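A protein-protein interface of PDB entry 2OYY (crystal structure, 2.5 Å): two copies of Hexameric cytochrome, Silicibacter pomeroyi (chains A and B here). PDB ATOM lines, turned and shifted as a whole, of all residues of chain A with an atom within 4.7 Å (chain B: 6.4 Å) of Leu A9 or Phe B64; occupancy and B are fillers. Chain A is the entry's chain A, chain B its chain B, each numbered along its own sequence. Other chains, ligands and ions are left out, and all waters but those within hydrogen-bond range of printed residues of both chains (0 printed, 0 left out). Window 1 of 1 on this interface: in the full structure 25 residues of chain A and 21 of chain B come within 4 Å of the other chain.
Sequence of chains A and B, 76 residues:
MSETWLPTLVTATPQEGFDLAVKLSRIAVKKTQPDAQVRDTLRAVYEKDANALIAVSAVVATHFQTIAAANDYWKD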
ATOM      1  N   LEU A   6     -34.420 -10.673 -10.764  1.00  0.00           N
ATOM      2  CA  LEU A   6     -32.984 -10.935 -10.950  1.00  0.00           C
ATOM      3  C   LEU A   6     -32.522 -10.929 -12.411  1.00  0.00           C
ATOM      4  O   LEU A   6     -32.340 -12.005 -13.003  1.00  0.00           O
ATOM      5  CB  LEU A   6     -32.537 -12.216 -10.247  1.00  0.00           C
ATOM      6  CG  LEU A   6     -31.039 -12.262  -9.919  1.00  0.00           C
ATOM      7  CD1 LEU A   6     -30.602 -11.091  -9.027  1.00  0.00           C
ATOM      8  CD2 LEU A   6     -30.649 -13.578  -9.287  1.00  0.00           C
ATOM      9  N   THR A   8     -29.587  -9.685 -13.850  1.00  0.00           N
ATOM     10  CA  THR A   8     -28.185 -10.074 -14.004  1.00  0.00           C
ATOM     11  C   THR A   8     -27.431 -10.100 -12.693  1.00  0.00           C
ATOM     12  O   THR A   8     -27.895  -9.601 -11.665  1.00  0.00           O
ATOM     13  CB  THR A   8     -27.396  -9.108 -14.916  1.00  0.00           C
ATOM     14  OG1 THR A   8     -27.552  -7.770 -14.431  1.00  0.00           O
ATOM     15  CG2 THR A   8     -27.834  -9.212 -16.389  1.00  0.00           C
ATOM     16  N   LEU A   9     -26.238 -10.680 -12.764  1.00  0.00           N
ATOM     17  CA  LEU A   9     -25.313 -10.748 -11.659  1.00  0.00           C
ATOM     18  C   LEU A   9     -24.223  -9.741 -11.911  1.00  0.00           C
ATOM     19  O   LEU A   9     -23.377  -9.496 -11.050  1.00  0.00           O
ATOM     20  CB  LEU A   9     -24.670 -12.124 -11.594  1.00  0.00           C
ATOM     21  CG  LEU A   9     -25.498 -13.377 -11.384  1.00  0.00           C
ATOM     22  CD1 LEU A   9     -24.530 -14.570 -11.458  1.00  0.00           C
ATOM     23  CD2 LEU A   9     -26.229 -13.312 -10.044  1.00  0.00           C
ATOM     24  N   VAL A  10     -24.214  -9.176 -13.106  1.00  0.00           N
ATOM     25  CA  VAL A  10     -23.221  -8.161 -13.427  1.00  0.00           C
ATOM     26  C   VAL A  10     -23.518  -6.912 -12.580  1.00  0.00           C
ATOM     27  O   VAL A  10     -24.652  -6.431 -12.521  1.00  0.00           O
ATOM     28  CB  VAL A  10     -23.160  -7.869 -14.929  1.00  0.00           C
ATOM     29  CG1 VAL A  10     -22.082  -6.853 -15.236  1.00  0.00           C
ATOM     30  CG2 VAL A  10     -22.914  -9.169 -15.701  1.00  0.00           C
ATOM     31  N   THR A  11     -22.479  -6.436 -11.899  1.00  0.00           N
ATOM     32  CA  THR A  11     -22.562  -5.348 -10.945  1.00  0.00           C
ATOM     33  C   THR A  11     -21.438  -4.340 -11.243  1.00  0.00           C
ATOM     34  O   THR A  11     -20.291  -4.739 -11.450  1.00  0.00           O
ATOM     35  CB  THR A  11     -22.449  -5.924  -9.510  1.00  0.00           C
ATOM     36  OG1 THR A  11     -23.758  -6.096  -8.935  1.00  0.00           O
ATOM     37  CG2 THR A  11     -21.642  -5.027  -8.639  1.00  0.00           C
ATOM     38  N   LEU A  20     -25.952  -6.858  -3.800  1.00  0.00           N
ATOM     39  CA  LEU A  20     -26.669  -7.844  -4.588  1.00  0.00           C
ATOM     40  C   LEU A  20     -26.620  -9.173  -3.856  1.00  0.00           C
ATOM     41  O   LEU A  20     -27.573  -9.938  -3.911  1.00  0.00           O
ATOM     42  CB  LEU A  20     -26.104  -7.957  -6.018  1.00  0.00           C
ATOM     43  CG  LEU A  20     -26.760  -9.001  -6.938  1.00  0.00           C
ATOM     44  CD1 LEU A  20     -28.252  -8.819  -7.004  1.00  0.00           C
ATOM     45  CD2 LEU A  20     -26.168  -9.021  -8.346  1.00  0.00           C
ATOM     46  N   LEU A  24     -29.669 -11.418  -2.742  1.00  0.00           N
ATOM     47  CA  LEU A  24     -29.843 -12.822  -3.089  1.00  0.00           C
ATOM     48  C   LEU A  24     -30.131 -13.719  -1.886  1.00  0.00           C
ATOM     49  O   LEU A  24     -30.828 -14.732  -2.007  1.00  0.00           O
ATOM     50  CB  LEU A  24     -28.632 -13.333  -3.861  1.00  0.00           C
ATOM     51  CG  LEU A  24     -28.573 -12.918  -5.334  1.00  0.00           C
ATOM     52  CD1 LEU A  24     -27.547 -13.757  -6.075  1.00  0.00           C
ATOM     53  CD2 LEU A  24     -29.933 -13.035  -6.020  1.00  0.00           C
ATOM     54  N   HIS A  63     -22.876 -16.135  -1.476  1.00  0.00           N
ATOM     55  CA  HIS A  63     -23.386 -15.405  -2.623  1.00  0.00           C
ATOM     56  C   HIS A  63     -22.357 -14.424  -3.190  1.00  0.00           C
ATOM     57  O   HIS A  63     -22.135 -14.394  -4.407  1.00  0.00           O
ATOM     58  CB  HIS A  63     -24.680 -14.669  -2.274  1.00  0.00           C
ATOM     59  CG  HIS A  63     -25.897 -15.529  -2.340  1.00  0.00           C
ATOM     60  ND1 HIS A  63     -26.325 -16.119  -3.508  1.00  0.00           N
ATOM     61  CD2 HIS A  63     -26.783 -15.894  -1.385  1.00  0.00           C
ATOM     62  CE1 HIS A  63     -27.427 -16.802  -3.277  1.00  0.00           C
ATOM     63  NE2 HIS A  63     -27.727 -16.682  -1.998  1.00  0.00           N
ATOM     64  N   THR A  66     -20.132 -15.981  -5.559  1.00  0.00           N
ATOM     65  CA  THR A  66     -20.743 -16.235  -6.860  1.00  0.00           C
ATOM     66  C   THR A  66     -20.799 -14.986  -7.721  1.00  0.00           C
ATOM     67  O   THR A  66     -20.528 -15.052  -8.918  1.00  0.00           O
ATOM     68  CB  THR A  66     -22.178 -16.804  -6.706  1.00  0.00           C
ATOM     69  OG1 THR A  66     -22.173 -17.857  -5.730  1.00  0.00           O
ATOM     70  CG2 THR A  66     -22.723 -17.325  -8.055  1.00  0.00           C
ATOM     71  N   ILE A  67     -21.154 -13.848  -7.127  1.00  0.00           N
ATOM     72  CA  ILE A  67     -21.233 -12.608  -7.900  1.00  0.00           C
ATOM     73  C   ILE A  67     -19.880 -11.914  -8.166  1.00  0.00           C
ATOM     74  O   ILE A  67     -19.729 -11.172  -9.137  1.00  0.00           O
ATOM     75  CB  ILE A  67     -22.319 -11.626  -7.377  1.00  0.00           C
ATOM     76  CG1 ILE A  67     -21.763 -10.217  -7.321  1.00  0.00           C
ATOM     77  CG2 ILE A  67     -22.807 -12.026  -6.016  1.00  0.00           C
ATOM     78  CD1 ILE A  67     -22.696  -9.228  -7.828  1.00  0.00           C
ATOM     79  N   ALA A  70     -18.837 -13.649 -11.079  1.00  0.00           N
ATOM     80  CA  ALA A  70     -19.637 -13.204 -12.219  1.00  0.00           C
ATOM     81  C   ALA A  70     -19.037 -11.936 -12.842  1.00  0.00           C
ATOM     82  O   ALA A  70     -19.060 -11.755 -14.052  1.00  0.00           O
ATOM     83  CB  ALA A  70     -21.095 -12.996 -11.812  1.00  0.00           C
ATOM     84  N   ASN A  71     -18.473 -11.080 -12.001  1.00  0.00           N
ATOM     85  CA  ASN A  71     -17.854  -9.834 -12.451  1.00  0.00           C
ATOM     86  C   ASN A  71     -16.346  -9.924 -12.681  1.00  0.00           C
ATOM     87  O   ASN A  71     -15.681  -8.896 -12.790  1.00  0.00           O
ATOM     88  CB  ASN A  71     -18.153  -8.711 -11.452  1.00  0.00           C
ATOM     89  CG  ASN A  71     -19.614  -8.389 -11.381  1.00  0.00           C
ATOM     90  OD1 ASN A  71     -20.367  -8.989 -10.601  1.00  0.00           O
ATOM     91  ND2 ASN A  71     -20.040  -7.448 -12.213  1.00  0.00           N
ATOM     92  N   PRO B  14     -30.541 -15.509 -14.934  1.00  0.00           N
ATOM     93  CA  PRO B  14     -30.167 -15.705 -13.529  1.00  0.00           C
ATOM     94  C   PRO B  14     -31.365 -15.959 -12.631  1.00  0.00           C
ATOM     95  O   PRO B  14     -31.255 -16.679 -11.647  1.00  0.00           O
ATOM     96  CB  PRO B  14     -29.531 -14.366 -13.156  1.00  0.00           C
ATOM     97  CG  PRO B  14     -28.992 -13.858 -14.402  1.00  0.00           C
ATOM     98  CD  PRO B  14     -30.008 -14.229 -15.436  1.00  0.00           C
ATOM     99  N   GLN B  15     -32.497 -15.363 -12.967  1.00  0.00           N
ATOM    100  CA  GLN B  15     -33.709 -15.548 -12.197  1.00  0.00           C
ATOM    101  C   GLN B  15     -34.087 -17.028 -12.141  1.00  0.00           C
ATOM    102  O   GLN B  15     -34.301 -17.601 -11.061  1.00  0.00           O
ATOM    103  CB  GLN B  15     -34.829 -14.732 -12.830  1.00  0.00           C
ATOM    104  CG  GLN B  15     -35.918 -14.363 -11.868  1.00  0.00           C
ATOM    105  CD  GLN B  15     -36.537 -13.017 -12.171  1.00  0.00           C
ATOM    106  OE1 GLN B  15     -35.841 -12.026 -12.415  1.00  0.00           O
ATOM    107  NE2 GLN B  15     -37.860 -12.969 -12.139  1.00  0.00           N
ATOM    108  N   GLU B  16     -34.158 -17.636 -13.320  1.00  0.00           N
ATOM    109  CA  GLU B  16     -34.431 -19.067 -13.461  1.00  0.00           C
ATOM    110  C   GLU B  16     -33.259 -19.906 -12.978  1.00  0.00           C
ATOM    111  O   GLU B  16     -33.376 -21.112 -12.833  1.00  0.00           O
ATOM    112  CB  GLU B  16     -34.735 -19.414 -14.913  1.00  0.00           C
ATOM    113  CG  GLU B  16     -35.806 -18.569 -15.540  1.00  0.00           C
ATOM    114  CD  GLU B  16     -35.923 -18.830 -17.012  1.00  0.00           C
ATOM    115  OE1 GLU B  16     -36.940 -18.408 -17.609  1.00  0.00           O
ATOM    116  OE2 GLU B  16     -34.995 -19.479 -17.574  1.00  0.00           O
ATOM    117  N   GLY B  17     -32.121 -19.263 -12.759  1.00  0.00           N
ATOM    118  CA  GLY B  17     -30.982 -19.924 -12.140  1.00  0.00           C
ATOM    119  C   GLY B  17     -31.262 -20.092 -10.659  1.00  0.00           C
ATOM    120  O   GLY B  17     -30.931 -21.115 -10.060  1.00  0.00           O
ATOM    121  N   PHE B  18     -31.901 -19.079 -10.083  1.00  0.00           N
ATOM    122  CA  PHE B  18     -32.140 -19.041  -8.660  1.00  0.00           C
ATOM    123  C   PHE B  18     -33.300 -19.960  -8.312  1.00  0.00           C
ATOM    124  O   PHE B  18     -33.277 -20.613  -7.272  1.00  0.00           O
ATOM    125  CB  PHE B  18     -32.414 -17.609  -8.221  1.00  0.00           C
ATOM    126  CG  PHE B  18     -32.271 -17.392  -6.752  1.00  0.00           C
ATOM    127  CD1 PHE B  18     -31.062 -16.980  -6.225  1.00  0.00           C
ATOM    128  CD2 PHE B  18     -33.343 -17.584  -5.904  1.00  0.00           C
ATOM    129  CE1 PHE B  18     -30.920 -16.777  -4.873  1.00  0.00           C
ATOM    130  CE2 PHE B  18     -33.214 -17.389  -4.547  1.00  0.00           C
ATOM    131  CZ  PHE B  18     -32.009 -16.987  -4.023  1.00  0.00           C
ATOM    132  N   ASP B  19     -34.290 -20.020  -9.204  1.00  0.00           N
ATOM    133  CA  ASP B  19     -35.462 -20.868  -9.024  1.00  0.00           C
ATOM    134  C   ASP B  19     -35.040 -22.349  -9.054  1.00  0.00           C
ATOM    135  O   ASP B  19     -35.460 -23.150  -8.201  1.00  0.00           O
ATOM    136  CB  ASP B  19     -36.505 -20.604 -10.135  1.00  0.00           C
ATOM    137  CG  ASP B  19     -37.289 -19.281  -9.949  1.00  0.00           C
ATOM    138  OD1 ASP B  19     -37.638 -18.908  -8.807  1.00  0.00           O
ATOM    139  OD2 ASP B  19     -37.590 -18.632 -10.967  1.00  0.00           O
ATOM    140  N   ALA B  21     -32.003 -23.387  -8.479  1.00  0.00           N
ATOM    141  CA  ALA B  21     -31.188 -23.578  -7.283  1.00  0.00           C
ATOM    142  C   ALA B  21     -32.109 -23.966  -6.131  1.00  0.00           C
ATOM    143  O   ALA B  21     -31.902 -24.986  -5.498  1.00  0.00           O
ATOM    144  CB  ALA B  21     -30.392 -22.340  -6.967  1.00  0.00           C
ATOM    145  N   VAL B  22     -33.170 -23.196  -5.922  1.00  0.00           N
ATOM    146  CA  VAL B  22     -34.167 -23.519  -4.904  1.00  0.00           C
ATOM    147  C   VAL B  22     -34.734 -24.932  -5.073  1.00  0.00           C
ATOM    148  O   VAL B  22     -34.812 -25.691  -4.090  1.00  0.00           O
ATOM    149  CB  VAL B  22     -35.314 -22.494  -4.905  1.00  0.00           C
ATOM    150  CG1 VAL B  22     -36.349 -22.817  -3.796  1.00  0.00           C
ATOM    151  CG2 VAL B  22     -34.752 -21.096  -4.745  1.00  0.00           C
ATOM    152  N   VAL B  59     -28.127 -23.332   1.722  1.00  0.00           N
ATOM    153  CA  VAL B  59     -28.192 -24.444   0.758  1.00  0.00           C
ATOM    154  C   VAL B  59     -28.394 -23.947  -0.688  1.00  0.00           C
ATOM    155  O   VAL B  59     -27.667 -24.355  -1.598  1.00  0.00           O
ATOM    156  CB  VAL B  59     -29.312 -25.432   1.076  1.00  0.00           C
ATOM    157  CG1 VAL B  59     -29.396 -26.487  -0.005  1.00  0.00           C
ATOM    158  CG2 VAL B  59     -29.079 -26.074   2.397  1.00  0.00           C
ATOM    159  N   VAL B  60     -29.382 -23.069  -0.879  1.00  0.00           N
ATOM    160  CA  VAL B  60     -29.650 -22.545  -2.202  1.00  0.00           C
ATOM    161  C   VAL B  60     -28.481 -21.675  -2.669  1.00  0.00           C
ATOM    162  O   VAL B  60     -28.217 -21.576  -3.862  1.00  0.00           O
ATOM    163  CB  VAL B  60     -31.092 -21.856  -2.381  1.00  0.00           C
ATOM    164  CG1 VAL B  60     -32.055 -22.181  -1.224  1.00  0.00           C
ATOM    165  CG2 VAL B  60     -30.997 -20.359  -2.642  1.00  0.00           C
ATOM    166  N   ALA B  61     -27.751 -21.087  -1.728  1.00  0.00           N
ATOM    167  CA  ALA B  61     -26.624 -20.222  -2.081  1.00  0.00           C
ATOM    168  C   ALA B  61     -25.478 -21.069  -2.632  1.00  0.00           C
ATOM    169  O   ALA B  61     -24.756 -20.646  -3.556  1.00  0.00           O
ATOM    170  CB  ALA B  61     -26.177 -19.391  -0.867  1.00  0.00           C
ATOM    171  N   THR B  62     -25.320 -22.266  -2.068  1.00  0.00           N
ATOM    172  CA  THR B  62     -24.376 -23.230  -2.601  1.00  0.00           C
ATOM    173  C   THR B  62     -24.825 -23.713  -3.973  1.00  0.00           C
ATOM    174  O   THR B  62     -24.002 -23.870  -4.879  1.00  0.00           O
ATOM    175  CB  THR B  62     -24.227 -24.456  -1.682  1.00  0.00           C
ATOM    176  OG1 THR B  62     -23.781 -24.041  -0.399  1.00  0.00           O
ATOM    177  CG2 THR B  62     -23.218 -25.440  -2.246  1.00  0.00           C
ATOM    178  N   HIS B  63     -26.119 -23.974  -4.124  1.00  0.00           N
ATOM    179  CA  HIS B  63     -26.641 -24.526  -5.374  1.00  0.00           C
ATOM    180  C   HIS B  63     -26.547 -23.498  -6.496  1.00  0.00           C
ATOM    181  O   HIS B  63     -26.091 -23.798  -7.592  1.00  0.00           O
ATOM    182  CB  HIS B  63     -28.086 -25.024  -5.210  1.00  0.00           C
ATOM    183  CG  HIS B  63     -28.199 -26.474  -4.839  1.00  0.00           C
ATOM    184  ND1 HIS B  63     -27.588 -27.482  -5.557  1.00  0.00           N
ATOM    185  CD2 HIS B  63     -28.896 -27.087  -3.851  1.00  0.00           C
ATOM    186  CE1 HIS B  63     -27.874 -28.648  -5.004  1.00  0.00           C
ATOM    187  NE2 HIS B  63     -28.662 -28.436  -3.963  1.00  0.00           N
ATOM    188  N   PHE B  64     -26.966 -22.277  -6.194  1.00  0.00           N
ATOM    189  CA  PHE B  64     -26.922 -21.170  -7.146  1.00  0.00           C
ATOM    190  C   PHE B  64     -25.513 -20.944  -7.671  1.00  0.00           C
ATOM    191  O   PHE B  64     -25.323 -20.618  -8.856  1.00  0.00           O
ATOM    192  CB  PHE B  64     -27.478 -19.891  -6.531  1.00  0.00           C
ATOM    193  CG  PHE B  64     -27.576 -18.775  -7.492  1.00  0.00           C
ATOM    194  CD1 PHE B  64     -28.507 -18.814  -8.525  1.00  0.00           C
ATOM    195  CD2 PHE B  64     -26.739 -17.684  -7.392  1.00  0.00           C
ATOM    196  CE1 PHE B  64     -28.602 -17.785  -9.445  1.00  0.00           C
ATOM    197  CE2 PHE B  64     -26.828 -16.641  -8.303  1.00  0.00           C
ATOM    198  CZ  PHE B  64     -27.767 -16.691  -9.325  1.00  0.00           C
ATOM    199  N   GLN B  65     -24.545 -21.166  -6.781  1.00  0.00           N
ATOM    200  CA  GLN B  65     -23.113 -21.089  -7.091  1.00  0.00           C
ATOM    201  C   GLN B  65     -22.684 -22.079  -8.197  1.00  0.00           C
ATOM    202  O   GLN B  65     -21.838 -21.761  -9.038  1.00  0.00           O
ATOM    203  CB  GLN B  65     -22.313 -21.312  -5.810  1.00  0.00           C
ATOM    204  CG  GLN B  65     -20.810 -21.227  -5.930  1.00  0.00           C
ATOM    205  CD  GLN B  65     -20.168 -20.888  -4.595  1.00  0.00           C
ATOM    206  OE1 GLN B  65     -20.322 -19.770  -4.101  1.00  0.00           O
ATOM    207  NE2 GLN B  65     -19.456 -21.851  -3.997  1.00  0.00           N
ATOM    208  N   THR B  66     -23.304 -23.260  -8.171  1.00  0.00           N
ATOM    209  CA  THR B  66     -23.055 -24.348  -9.115  1.00  0.00           C
ATOM    210  C   THR B  66     -23.652 -24.037 -10.476  1.00  0.00           C
ATOM    211  O   THR B  66     -22.954 -24.037 -11.485  1.00  0.00           O
ATOM    212  CB  THR B  66     -23.671 -25.664  -8.603  1.00  0.00           C
ATOM    213  OG1 THR B  66     -23.270 -25.891  -7.250  1.00  0.00           O
ATOM    214  CG2 THR B  66     -23.222 -26.825  -9.443  1.00  0.00           C
ATOM    215  N   ILE B  67     -24.952 -23.756 -10.496  1.00  0.00           N
ATOM    216  CA  ILE B  67     -25.641 -23.468 -11.749  1.00  0.00           C
ATOM    217  C   ILE B  67     -25.142 -22.168 -12.390  1.00  0.00           C
ATOM    218  O   ILE B  67     -24.916 -22.118 -13.601  1.00  0.00           O
ATOM    219  CB  ILE B  67     -27.192 -23.564 -11.618  1.00  0.00           C
ATOM    220  CG1 ILE B  67     -27.894 -22.384 -12.273  1.00  0.00           C
ATOM    221  CG2 ILE B  67     -27.630 -23.660 -10.165  1.00  0.00           C
ATOM    222  CD1 ILE B  67     -29.350 -22.594 -12.396  1.00  0.00           C
ATOM    223  N   ALA B  68     -24.936 -21.135 -11.574  1.00  0.00           N
ATOM    224  CA  ALA B  68     -24.403 -19.867 -12.075  1.00  0.00           C
ATOM    225  C   ALA B  68     -23.119 -20.111 -12.860  1.00  0.00           C
ATOM    226  O   ALA B  68     -22.922 -19.545 -13.938  1.00  0.00           O
ATOM    227  CB  ALA B  68     -24.163 -18.890 -10.927  1.00  0.00           C
ATOM    228  N   ALA B  69     -22.267 -20.977 -12.313  1.00  0.00           N
ATOM    229  CA  ALA B  69     -21.012 -21.387 -12.958  1.00  0.00           C
ATOM    230  C   ALA B  69     -21.290 -22.168 -14.223  1.00  0.00           C
ATOM    231  O   ALA B  69     -20.565 -22.035 -15.200  1.00  0.00           O
ATOM    232  CB  ALA B  69     -20.158 -22.224 -11.992  1.00  0.00           C
ATOM    233  N   TYR B  73     -22.293 -17.608 -15.804  1.00  0.00           N
ATOM    234  CA  TYR B  73     -22.691 -16.412 -15.070  1.00  0.00           C
ATOM    235  C   TYR B  73     -23.651 -15.445 -15.791  1.00  0.00           C
ATOM    236  O   TYR B  73     -23.891 -14.346 -15.309  1.00  0.00           O
ATOM    237  CB  TYR B  73     -21.446 -15.712 -14.480  1.00  0.00           C
ATOM    238  CG  TYR B  73     -20.681 -16.585 -13.496  1.00  0.00           C
ATOM    239  CD1 TYR B  73     -21.145 -16.757 -12.184  1.00  0.00           C
ATOM    240  CD2 TYR B  73     -19.513 -17.254 -13.869  1.00  0.00           C
ATOM    241  CE1 TYR B  73     -20.465 -17.562 -11.273  1.00  0.00           C
ATOM    242  CE2 TYR B  73     -18.809 -18.066 -12.948  1.00  0.00           C
ATOM    243  CZ  TYR B  73     -19.298 -18.217 -11.655  1.00  0.00           C
ATOM    244  OH  TYR B  73     -18.644 -19.021 -10.723  1.00  0.00           O
ATOM    245  N   TRP B  74     -24.240 -15.882 -16.905  1.00  0.00           N
ATOM    246  CA  TRP B  74     -25.140 -15.045 -17.740  1.00  0.00           C
ATOM    247  C   TRP B  74     -24.536 -13.698 -18.150  1.00  0.00           C
ATOM    248  O   TRP B  74     -23.704 -13.629 -19.056  1.00  0.00           O
ATOM    249  CB  TRP B  74     -26.491 -14.807 -17.047  1.00  0.00           C
ATOM    250  CG  TRP B  74     -27.199 -16.069 -16.607  1.00  0.00           C
ATOM    251  CD1 TRP B  74     -28.039 -16.849 -17.358  1.00  0.00           C
ATOM    252  CD2 TRP B  74     -27.135 -16.679 -15.318  1.00  0.00           C
ATOM    253  NE1 TRP B  74     -28.495 -17.914 -16.614  1.00  0.00           N
ATOM    254  CE2 TRP B  74     -27.961 -17.835 -15.358  1.00  0.00           C
ATOM    255  CE3 TRP B  74     -26.463 -16.369 -14.127  1.00  0.00           C
ATOM    256  CZ2 TRP B  74     -28.132 -18.683 -14.246  1.00  0.00           C
ATOM    257  CZ3 TRP B  74     -26.629 -17.222 -13.023  1.00  0.00           C
ATOM    258  CH2 TRP B  74     -27.465 -18.358 -13.095  1.00  0.00           C
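The side-chain amide oxygen of Gln B15 lies within hydrogen-bond range of the backbone NH of Leu A6. The side-chain amide oxygen (OE1) of Gln B65 is in hydrogen-bond range of the side-chain hydroxyl (OG1) of Thr A66.
The backbone carbonyl oxygen (O) of Ala B68 sits at hydrogen-bond distance from the backbone NH (N) of Tyr B73 (2.8 Å). The backbone carbonyl oxygen of Leu A9 lies close to the side-chain amide oxygen of Asn A71.
Among the printed residues, merely in contact across the chains: Leu A6 with Pro B14, Thr A8 with Pro B14, Leu A9 with Phe B64, Leu A9 with Tyr B73, Leu A9 with Trp B74, Leu A24 with Phe B18, Leu A24 with Phe B64, His A63 with Phe B18, His A63 with Ala B61, Thr A66 with Ala B68, Thr A66 with Tyr B73 and Ala A70 with Tyr B73.
Of chain B, only Phe B64, Tyr B73 and Trp B74 come within 4 Å of Leu A9. Printed residues of chain A within 4 Å of Phe B64: Leu A9 and Leu A24. Of the printed residues of chain A, Tyr B73 touches Leu A9 (3.9 Å), Thr A66 (3.4 Å) and Ala A70 (3.8 Å). Of the printed residues of chain A, Gln B65 touches Thr A66. Of the printed residues of chain B, Thr A8 touches Pro B14 (3.9 Å). Printed residues of chain A within 4 Å of Ala B61: His A63. Printed residues of chain A within 4 Å of Phe B18: Leu A24 and His A63. Asn A71 touches none of the printed residues of chain B. Val B59 touches none of the printed residues of chain A. The nearest residue of chain B that does not touch Leu A9 is Ala B68 (4.4 Å). The nearest residue of chain A that does not touch Phe B64 is Thr A66 (4.1 Å). The nearest printed residue of chain A that does not touch Ala B68 is Leu A9 (4.4 Å).
Printed residues of chain A that touch a printed residue of chain B: Leu A6, Thr A8, Leu A9, Leu A24, His A63, Thr A66 and Ala A70. Hydrophobic or aromatic side chains of chain A within 4 Å of the printed part of chain B: Leu A6, Leu A9, Leu A24, His A63 and Ala A70. Along chain A the printed residues that touch a printed residue of chain B span positions 6 to 70. Printed residues of chain B that touch a printed residue of chain A: Pro B14, Gln B15, Phe B18, Ala B61, Phe B64, Gln B65, Ala B68, Tyr B73 and Trp B74. Among the printed residues, 14 pairs touch across the chains.
Positions printed for both chains: 63, 66 and 67. Of the 14 pairs that touch across the chains among the printed residues, none has its exchanged pair printed and touching as well.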
